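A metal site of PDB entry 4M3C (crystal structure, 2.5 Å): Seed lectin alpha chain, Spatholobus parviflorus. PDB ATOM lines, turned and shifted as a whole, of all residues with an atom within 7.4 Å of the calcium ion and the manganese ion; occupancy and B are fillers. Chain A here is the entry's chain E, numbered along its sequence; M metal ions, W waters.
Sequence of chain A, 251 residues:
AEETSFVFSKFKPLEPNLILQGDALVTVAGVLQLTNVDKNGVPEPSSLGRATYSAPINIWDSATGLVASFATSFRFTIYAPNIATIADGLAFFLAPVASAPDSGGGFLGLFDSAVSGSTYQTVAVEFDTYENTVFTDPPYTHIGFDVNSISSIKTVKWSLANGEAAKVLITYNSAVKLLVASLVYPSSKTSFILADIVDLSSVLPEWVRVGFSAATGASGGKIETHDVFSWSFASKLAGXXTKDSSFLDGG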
ATOM      1  N   ASP A  88      23.503  -8.371 -10.381  1.00  0.00           N
ATOM      2  CA  ASP A  88      22.193  -7.922 -10.872  1.00  0.00           C
ATOM      3  C   ASP A  88      21.031  -8.330  -9.952  1.00  0.00           C
ATOM      4  O   ASP A  88      19.932  -7.768 -10.092  1.00  0.00           O
ATOM      5  CB  ASP A  88      21.898  -8.460 -12.275  1.00  0.00           C
ATOM      6  CG  ASP A  88      22.550  -7.647 -13.368  1.00  0.00           C
ATOM      7  OD1 ASP A  88      23.776  -7.724 -13.502  1.00  0.00           O
ATOM      8  OD2 ASP A  88      21.828  -6.959 -14.111  1.00  0.00           O
ATOM      9  N   GLY A  89      21.272  -9.288  -9.048  1.00  0.00           N
ATOM     10  CA  GLY A  89      20.237  -9.834  -8.214  1.00  0.00           C
ATOM     11  C   GLY A  89      20.223 -11.356  -8.031  1.00  0.00           C
ATOM     12  O   GLY A  89      21.091 -12.105  -8.516  1.00  0.00           O
ATOM     13  N   GLY A 105      23.855 -12.181 -16.202  1.00  0.00           N
ATOM     14  CA  GLY A 105      23.689 -10.731 -16.009  1.00  0.00           C
ATOM     15  C   GLY A 105      22.299 -10.410 -15.476  1.00  0.00           C
ATOM     16  O   GLY A 105      21.821 -11.040 -14.533  1.00  0.00           O
ATOM     17  N   GLY A 106      21.620  -9.466 -16.129  1.00  0.00           N
ATOM     18  CA  GLY A 106      20.272  -9.041 -15.735  1.00  0.00           C
ATOM     19  C   GLY A 106      19.135 -10.003 -16.011  1.00  0.00           C
ATOM     20  O   GLY A 106      17.959  -9.692 -15.745  1.00  0.00           O
ATOM     21  N   PHE A 107      19.469 -11.172 -16.513  1.00  0.00           N
ATOM     22  CA  PHE A 107      18.460 -12.175 -16.859  1.00  0.00           C
ATOM     23  C   PHE A 107      18.341 -13.109 -15.658  1.00  0.00           C
ATOM     24  O   PHE A 107      17.368 -13.849 -15.554  1.00  0.00           O
ATOM     25  CB  PHE A 107      18.831 -12.972 -18.145  1.00  0.00           C
ATOM     26  CG  PHE A 107      19.115 -12.104 -19.366  1.00  0.00           C
ATOM     27  CD1 PHE A 107      18.091 -11.664 -20.188  1.00  0.00           C
ATOM     28  CD2 PHE A 107      20.429 -11.731 -19.687  1.00  0.00           C
ATOM     29  CE1 PHE A 107      18.357 -10.855 -21.283  1.00  0.00           C
ATOM     30  CE2 PHE A 107      20.706 -10.934 -20.781  1.00  0.00           C
ATOM     31  CZ  PHE A 107      19.663 -10.495 -21.578  1.00  0.00           C
ATOM     32  N   LEU A 108      19.348 -13.079 -14.768  1.00  0.00           N
ATOM     33  CA  LEU A 108      19.306 -13.799 -13.488  1.00  0.00           C
ATOM     34  C   LEU A 108      19.214 -15.326 -13.635  1.00  0.00           C
ATOM     35  O   LEU A 108      18.756 -16.018 -12.718  1.00  0.00           O
ATOM     36  CB  LEU A 108      18.146 -13.282 -12.595  1.00  0.00           C
ATOM     37  CG  LEU A 108      17.849 -11.764 -12.514  1.00  0.00           C
ATOM     38  CD1 LEU A 108      16.539 -11.466 -11.768  1.00  0.00           C
ATOM     39  CD2 LEU A 108      19.017 -10.993 -11.893  1.00  0.00           C
ATOM     40  N   GLU A 126      11.902 -12.116  -7.712  1.00  0.00           N
ATOM     41  CA  GLU A 126      13.247 -11.628  -7.844  1.00  0.00           C
ATOM     42  C   GLU A 126      13.492 -10.459  -6.880  1.00  0.00           C
ATOM     43  O   GLU A 126      12.571  -9.718  -6.509  1.00  0.00           O
ATOM     44  CB  GLU A 126      13.461 -11.147  -9.283  1.00  0.00           C
ATOM     45  CG  GLU A 126      12.394 -10.138  -9.703  1.00  0.00           C
ATOM     46  CD  GLU A 126      12.870  -9.208 -10.829  1.00  0.00           C
ATOM     47  OE1 GLU A 126      13.478  -9.701 -11.819  1.00  0.00           O
ATOM     48  OE2 GLU A 126      12.630  -7.980 -10.737  1.00  0.00           O
ATOM     49  N   PHE A 127      14.757 -10.302  -6.552  1.00  0.00           N
ATOM     50  CA  PHE A 127      15.227  -9.279  -5.637  1.00  0.00           C
ATOM     51  C   PHE A 127      16.333  -8.728  -6.484  1.00  0.00           C
ATOM     52  O   PHE A 127      17.454  -9.229  -6.508  1.00  0.00           O
ATOM     53  CB  PHE A 127      15.719  -9.897  -4.321  1.00  0.00           C
ATOM     54  CG  PHE A 127      14.687 -10.739  -3.621  1.00  0.00           C
ATOM     55  CD1 PHE A 127      13.730 -10.158  -2.783  1.00  0.00           C
ATOM     56  CD2 PHE A 127      14.624 -12.097  -3.825  1.00  0.00           C
ATOM     57  CE1 PHE A 127      12.759 -10.913  -2.149  1.00  0.00           C
ATOM     58  CE2 PHE A 127      13.650 -12.871  -3.186  1.00  0.00           C
ATOM     59  CZ  PHE A 127      12.718 -12.274  -2.349  1.00  0.00           C
ATOM     60  N   ASP A 128      15.927  -7.687  -7.218  1.00  0.00           N
ATOM     61  CA  ASP A 128      16.628  -7.167  -8.358  1.00  0.00           C
ATOM     62  C   ASP A 128      17.420  -5.944  -7.958  1.00  0.00           C
ATOM     63  O   ASP A 128      16.905  -4.955  -7.430  1.00  0.00           O
ATOM     64  CB  ASP A 128      15.565  -6.825  -9.394  1.00  0.00           C
ATOM     65  CG  ASP A 128      16.144  -6.403 -10.719  1.00  0.00           C
ATOM     66  OD1 ASP A 128      15.343  -6.349 -11.669  1.00  0.00           O
ATOM     67  OD2 ASP A 128      17.364  -6.139 -10.832  1.00  0.00           O
ATOM     68  N   THR A 129      18.684  -5.980  -8.277  1.00  0.00           N
ATOM     69  CA  THR A 129      19.618  -5.112  -7.647  1.00  0.00           C
ATOM     70  C   THR A 129      20.184  -4.072  -8.644  1.00  0.00           C
ATOM     71  O   THR A 129      20.905  -3.144  -8.263  1.00  0.00           O
ATOM     72  CB  THR A 129      20.603  -6.029  -6.918  1.00  0.00           C
ATOM     73  OG1 THR A 129      20.680  -5.695  -5.523  1.00  0.00           O
ATOM     74  CG2 THR A 129      21.936  -6.132  -7.578  1.00  0.00           C
ATOM     75  N   TYR A 130      19.781  -4.168  -9.905  1.00  0.00           N
ATOM     76  CA  TYR A 130      20.278  -3.267 -10.926  1.00  0.00           C
ATOM     77  C   TYR A 130      19.159  -2.849 -11.904  1.00  0.00           C
ATOM     78  O   TYR A 130      18.462  -3.707 -12.451  1.00  0.00           O
ATOM     79  CB  TYR A 130      21.430  -3.928 -11.690  1.00  0.00           C
ATOM     80  CG  TYR A 130      21.921  -3.083 -12.852  1.00  0.00           C
ATOM     81  CD1 TYR A 130      23.036  -2.255 -12.712  1.00  0.00           C
ATOM     82  CD2 TYR A 130      21.266  -3.082 -14.079  1.00  0.00           C
ATOM     83  CE1 TYR A 130      23.503  -1.481 -13.759  1.00  0.00           C
ATOM     84  CE2 TYR A 130      21.711  -2.306 -15.130  1.00  0.00           C
ATOM     85  CZ  TYR A 130      22.843  -1.510 -14.979  1.00  0.00           C
ATOM     86  OH  TYR A 130      23.306  -0.724 -16.020  1.00  0.00           O
ATOM     87  N   GLU A 131      18.999  -1.539 -12.136  1.00  0.00           N
ATOM     88  CA  GLU A 131      17.987  -1.046 -13.075  1.00  0.00           C
ATOM     89  C   GLU A 131      18.365  -1.245 -14.560  1.00  0.00           C
ATOM     90  O   GLU A 131      19.202  -0.503 -15.133  1.00  0.00           O
ATOM     91  CB  GLU A 131      17.593   0.414 -12.795  1.00  0.00           C
ATOM     92  CG  GLU A 131      16.360   0.846 -13.589  1.00  0.00           C
ATOM     93  CD  GLU A 131      16.134   2.349 -13.684  1.00  0.00           C
ATOM     94  OE1 GLU A 131      16.980   3.152 -13.252  1.00  0.00           O
ATOM     95  OE2 GLU A 131      15.074   2.756 -14.206  1.00  0.00           O
ATOM     96  N   ASN A 132      17.732  -2.253 -15.158  1.00  0.00           N
ATOM     97  CA  ASN A 132      17.818  -2.489 -16.587  1.00  0.00           C
ATOM     98  C   ASN A 132      16.570  -1.876 -17.212  1.00  0.00           C
ATOM     99  O   ASN A 132      15.505  -2.493 -17.186  1.00  0.00           O
ATOM    100  CB  ASN A 132      17.845  -4.006 -16.859  1.00  0.00           C
ATOM    101  CG  ASN A 132      19.132  -4.680 -16.403  1.00  0.00           C
ATOM    102  OD1 ASN A 132      20.009  -4.959 -17.220  1.00  0.00           O
ATOM    103  ND2 ASN A 132      19.252  -4.944 -15.111  1.00  0.00           N
ATOM    104  N   THR A 133      16.701  -0.641 -17.747  1.00  0.00           N
ATOM    105  CA  THR A 133      15.579   0.085 -18.374  1.00  0.00           C
ATOM    106  C   THR A 133      15.139  -0.702 -19.581  1.00  0.00           C
ATOM    107  O   THR A 133      14.020  -0.573 -20.040  1.00  0.00           O
ATOM    108  CB  THR A 133      15.872   1.562 -18.828  1.00  0.00           C
ATOM    109  OG1 THR A 133      17.230   1.697 -19.273  1.00  0.00           O
ATOM    110  CG2 THR A 133      15.579   2.590 -17.730  1.00  0.00           C
ATOM    111  N   PHE A 135      14.378  -3.673 -19.373  1.00  0.00           N
ATOM    112  CA  PHE A 135      13.420  -4.665 -18.887  1.00  0.00           C
ATOM    113  C   PHE A 135      12.266  -3.985 -18.171  1.00  0.00           C
ATOM    114  O   PHE A 135      11.509  -4.614 -17.423  1.00  0.00           O
ATOM    115  CB  PHE A 135      14.113  -5.666 -17.952  1.00  0.00           C
ATOM    116  CG  PHE A 135      15.290  -6.399 -18.565  1.00  0.00           C
ATOM    117  CD1 PHE A 135      15.420  -6.549 -19.955  1.00  0.00           C
ATOM    118  CD2 PHE A 135      16.243  -6.988 -17.765  1.00  0.00           C
ATOM    119  CE1 PHE A 135      16.488  -7.246 -20.506  1.00  0.00           C
ATOM    120  CE2 PHE A 135      17.306  -7.689 -18.292  1.00  0.00           C
ATOM    121  CZ  PHE A 135      17.444  -7.815 -19.659  1.00  0.00           C
ATOM    122  N   THR A 136      12.104  -2.703 -18.433  1.00  0.00           N
ATOM    123  CA  THR A 136      11.277  -1.813 -17.605  1.00  0.00           C
ATOM    124  C   THR A 136      11.541  -2.005 -16.088  1.00  0.00           C
ATOM    125  O   THR A 136      10.599  -2.062 -15.282  1.00  0.00           O
ATOM    126  CB  THR A 136       9.763  -1.789 -18.020  1.00  0.00           C
ATOM    127  OG1 THR A 136       9.613  -2.059 -19.417  1.00  0.00           O
ATOM    128  CG2 THR A 136       9.124  -0.404 -17.713  1.00  0.00           C
ATOM    129  N   ASP A 137      12.828  -2.089 -15.703  1.00  0.00           N
ATOM    130  CA  ASP A 137      13.193  -1.955 -14.275  1.00  0.00           C
ATOM    131  C   ASP A 137      12.886  -0.573 -13.743  1.00  0.00           C
ATOM    132  O   ASP A 137      13.228   0.417 -14.391  1.00  0.00           O
ATOM    133  CB  ASP A 137      14.644  -2.265 -14.007  1.00  0.00           C
ATOM    134  CG  ASP A 137      14.893  -3.723 -13.925  1.00  0.00           C
ATOM    135  OD1 ASP A 137      13.886  -4.440 -13.960  1.00  0.00           O
ATOM    136  OD2 ASP A 137      16.046  -4.185 -13.809  1.00  0.00           O
ATOM    137  N   PRO A 138      12.214  -0.524 -12.565  1.00  0.00           N
ATOM    138  CA  PRO A 138      11.992   0.717 -11.862  1.00  0.00           C
ATOM    139  C   PRO A 138      13.327   1.166 -11.280  1.00  0.00           C
ATOM    140  O   PRO A 138      14.242   0.323 -11.143  1.00  0.00           O
ATOM    141  CB  PRO A 138      10.991   0.341 -10.741  1.00  0.00           C
ATOM    142  CG  PRO A 138      10.813  -1.135 -10.790  1.00  0.00           C
ATOM    143  CD  PRO A 138      11.817  -1.694 -11.758  1.00  0.00           C
ATOM    144  N   TYR A 140      14.660   2.050  -8.365  1.00  0.00           N
ATOM    145  CA  TYR A 140      15.249   1.650  -7.113  1.00  0.00           C
ATOM    146  C   TYR A 140      15.395   0.146  -7.078  1.00  0.00           C
ATOM    147  O   TYR A 140      14.738  -0.557  -7.812  1.00  0.00           O
ATOM    148  CB  TYR A 140      14.365   2.120  -5.955  1.00  0.00           C
ATOM    149  CG  TYR A 140      12.895   2.022  -6.278  1.00  0.00           C
ATOM    150  CD1 TYR A 140      12.239   0.802  -6.275  1.00  0.00           C
ATOM    151  CD2 TYR A 140      12.164   3.160  -6.612  1.00  0.00           C
ATOM    152  CE1 TYR A 140      10.889   0.710  -6.574  1.00  0.00           C
ATOM    153  CE2 TYR A 140      10.811   3.089  -6.908  1.00  0.00           C
ATOM    154  CZ  TYR A 140      10.179   1.869  -6.887  1.00  0.00           C
ATOM    155  OH  TYR A 140       8.845   1.806  -7.225  1.00  0.00           O
ATOM    156  N   HIS A 142      14.441  -3.369  -6.007  1.00  0.00           N
ATOM    157  CA  HIS A 142      13.011  -3.784  -5.980  1.00  0.00           C
ATOM    158  C   HIS A 142      12.797  -5.247  -5.917  1.00  0.00           C
ATOM    159  O   HIS A 142      13.679  -6.030  -6.235  1.00  0.00           O
ATOM    160  CB  HIS A 142      12.295  -3.247  -7.197  1.00  0.00           C
ATOM    161  CG  HIS A 142      12.966  -3.602  -8.507  1.00  0.00           C
ATOM    162  ND1 HIS A 142      13.953  -2.858  -9.046  1.00  0.00           N
ATOM    163  CD2 HIS A 142      12.789  -4.677  -9.378  1.00  0.00           C
ATOM    164  CE1 HIS A 142      14.378  -3.409 -10.191  1.00  0.00           C
ATOM    165  NE2 HIS A 142      13.669  -4.516 -10.402  1.00  0.00           N
ATOM    166  N   ILE A 143      11.601  -5.620  -5.468  1.00  0.00           N
ATOM    167  CA  ILE A 143      11.136  -7.008  -5.453  1.00  0.00           C
ATOM    168  C   ILE A 143      10.245  -7.034  -6.664  1.00  0.00           C
ATOM    169  O   ILE A 143       9.676  -6.021  -6.998  1.00  0.00           O
ATOM    170  CB  ILE A 143      10.291  -7.289  -4.173  1.00  0.00           C
ATOM    171  CG1 ILE A 143      11.164  -7.165  -2.922  1.00  0.00           C
ATOM    172  CG2 ILE A 143       9.645  -8.685  -4.199  1.00  0.00           C
ATOM    173  CD1 ILE A 143      10.393  -7.148  -1.610  1.00  0.00           C
ATOM    174  N   GLY A 144      10.114  -8.187  -7.312  1.00  0.00           N
ATOM    175  CA  GLY A 144       9.304  -8.279  -8.515  1.00  0.00           C
ATOM    176  C   GLY A 144       8.745  -9.674  -8.725  1.00  0.00           C
ATOM    177  O   GLY A 144       9.361 -10.691  -8.287  1.00  0.00           O
ATOM    178  N   ASP A 146       7.983 -12.229 -11.586  1.00  0.00           N
ATOM    179  CA  ASP A 146       8.336 -12.559 -12.987  1.00  0.00           C
ATOM    180  C   ASP A 146       7.491 -13.734 -13.484  1.00  0.00           C
ATOM    181  O   ASP A 146       7.564 -14.842 -12.922  1.00  0.00           O
ATOM    182  CB  ASP A 146       9.824 -12.863 -13.086  1.00  0.00           C
ATOM    183  CG  ASP A 146      10.670 -11.632 -12.741  1.00  0.00           C
ATOM    184  OD1 ASP A 146      10.057 -10.555 -12.517  1.00  0.00           O
ATOM    185  OD2 ASP A 146      11.942 -11.727 -12.703  1.00  0.00           O
ATOM    186  N   ILE A 150      11.104 -11.417 -17.723  1.00  0.00           N
ATOM    187  CA  ILE A 150      11.855 -10.595 -16.781  1.00  0.00           C
ATOM    188  C   ILE A 150      11.208  -9.179 -16.648  1.00  0.00           C
ATOM    189  O   ILE A 150      11.486  -8.436 -15.691  1.00  0.00           O
ATOM    190  CB  ILE A 150      13.323 -10.515 -17.239  1.00  0.00           C
ATOM    191  CG1 ILE A 150      14.240  -9.965 -16.133  1.00  0.00           C
ATOM    192  CG2 ILE A 150      13.429  -9.760 -18.538  1.00  0.00           C
ATOM    193  CD1 ILE A 150      14.894 -11.050 -15.313  1.00  0.00           C
ATOM    194  N   SER A 151      10.322  -8.789 -17.570  1.00  0.00           N
ATOM    195  CA  SER A 151       9.614  -7.540 -17.354  1.00  0.00           C
ATOM    196  C   SER A 151       8.538  -7.850 -16.315  1.00  0.00           C
ATOM    197  O   SER A 151       7.438  -8.307 -16.678  1.00  0.00           O
ATOM    198  CB  SER A 151       8.961  -6.978 -18.638  1.00  0.00           C
ATOM    199  OG  SER A 151       9.901  -6.298 -19.464  1.00  0.00           O
ATOM    200  N   SER A 152       8.890  -7.625 -15.037  1.00  0.00           N
ATOM    201  CA  SER A 152       8.033  -7.983 -13.907  1.00  0.00           C
ATOM    202  C   SER A 152       6.610  -7.487 -14.081  1.00  0.00           C
ATOM    203  O   SER A 152       6.354  -6.326 -14.434  1.00  0.00           O
ATOM    204  CB  SER A 152       8.602  -7.442 -12.587  1.00  0.00           C
ATOM    205  OG  SER A 152       9.931  -7.874 -12.390  1.00  0.00           O
ATOM    206  N   THR A 155       6.005  -4.764  -9.315  1.00  0.00           N
ATOM    207  CA  THR A 155       7.130  -4.527  -8.350  1.00  0.00           C
ATOM    208  C   THR A 155       6.786  -3.606  -7.131  1.00  0.00           C
ATOM    209  O   THR A 155       5.767  -2.921  -7.180  1.00  0.00           O
ATOM    210  CB  THR A 155       8.341  -3.882  -9.037  1.00  0.00           C
ATOM    211  OG1 THR A 155       7.965  -2.581  -9.547  1.00  0.00           O
ATOM    212  CG2 THR A 155       8.882  -4.804 -10.200  1.00  0.00           C
HETATM  213 CA    CA M   1      17.571  -5.814 -13.277  1.00  0.00          CA
HETATM  214 MN    MN M   2      13.600  -6.216 -12.312  1.00  0.00          MN
HETATM  215  O   HOH W   1      11.377  -6.005 -12.534  1.00  0.00           O
HETATM  216  O   HOH W   2      16.441  -7.629 -14.239  1.00  0.00           O
HETATM  217  O   HOH W   3      19.340  -6.692 -12.746  1.00  0.00           O
HETATM  218  O   HOH W   4      13.434  -7.995 -13.859  1.00  0.00           O
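The side-chain carboxylate (OE1) of Glu 126 sits close to the side-chain carboxylate (OD2) of Asp 146, at 2.7 Å. O of Tyr 140 sits at hydrogen-bond distance from ND1 of His 142. The backbone NH (N) of Glu 126 lies within hydrogen-bond range of the backbone carbonyl oxygen (O) of Gly 144 (3.0 Å). The side-chain amide nitrogen of Asn 132 sits close to the side-chain carboxylate of Asp 88 (3.4 Å). The side-chain hydroxyl (OG) of Ser 152 lies close to the side-chain carboxylate (OE2) of Glu 126 (3.2 Å).
The manganese ion is bound by the side-chain carboxylate of Asp 128 (1.9 Å), water W1 (2.2 Å), water W4 (2.4 Å), the side-chain carboxylate of Asp 137 (2.4 Å), the side-chain carboxylate of Glu 126 (2.6 Å) and a ring nitrogen (NE2) of His 142 (2.6 Å). The manganese ion has six donor atoms within binding distance.
The calcium ion is bound by water W3 (2.0 Å), the side-chain carboxylate (OD2) of Asp 137 (2.3 Å), water W2 (2.3 Å), the backbone carbonyl oxygen (O) of Tyr 130 (2.4 Å), the side-chain carboxylate (OD2) of Asp 128 (2.5 Å), the side-chain amide nitrogen (ND2) of Asn 132 (2.6 Å) and the side-chain carboxylate (OD1) of Asp 128 (2.8 Å). The calcium ion has seven donor atoms within binding distance.
Water W4 lies within hydrogen-bond range of the side-chain carboxylate of Glu 126 and the backbone carbonyl oxygen of Ile 150.
The nearest printed residue that does not touch the manganese ion is Ser 152 (4.03 Å).
Of the 27 residues printed, 4 come within 4 Å of the calcium ion.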
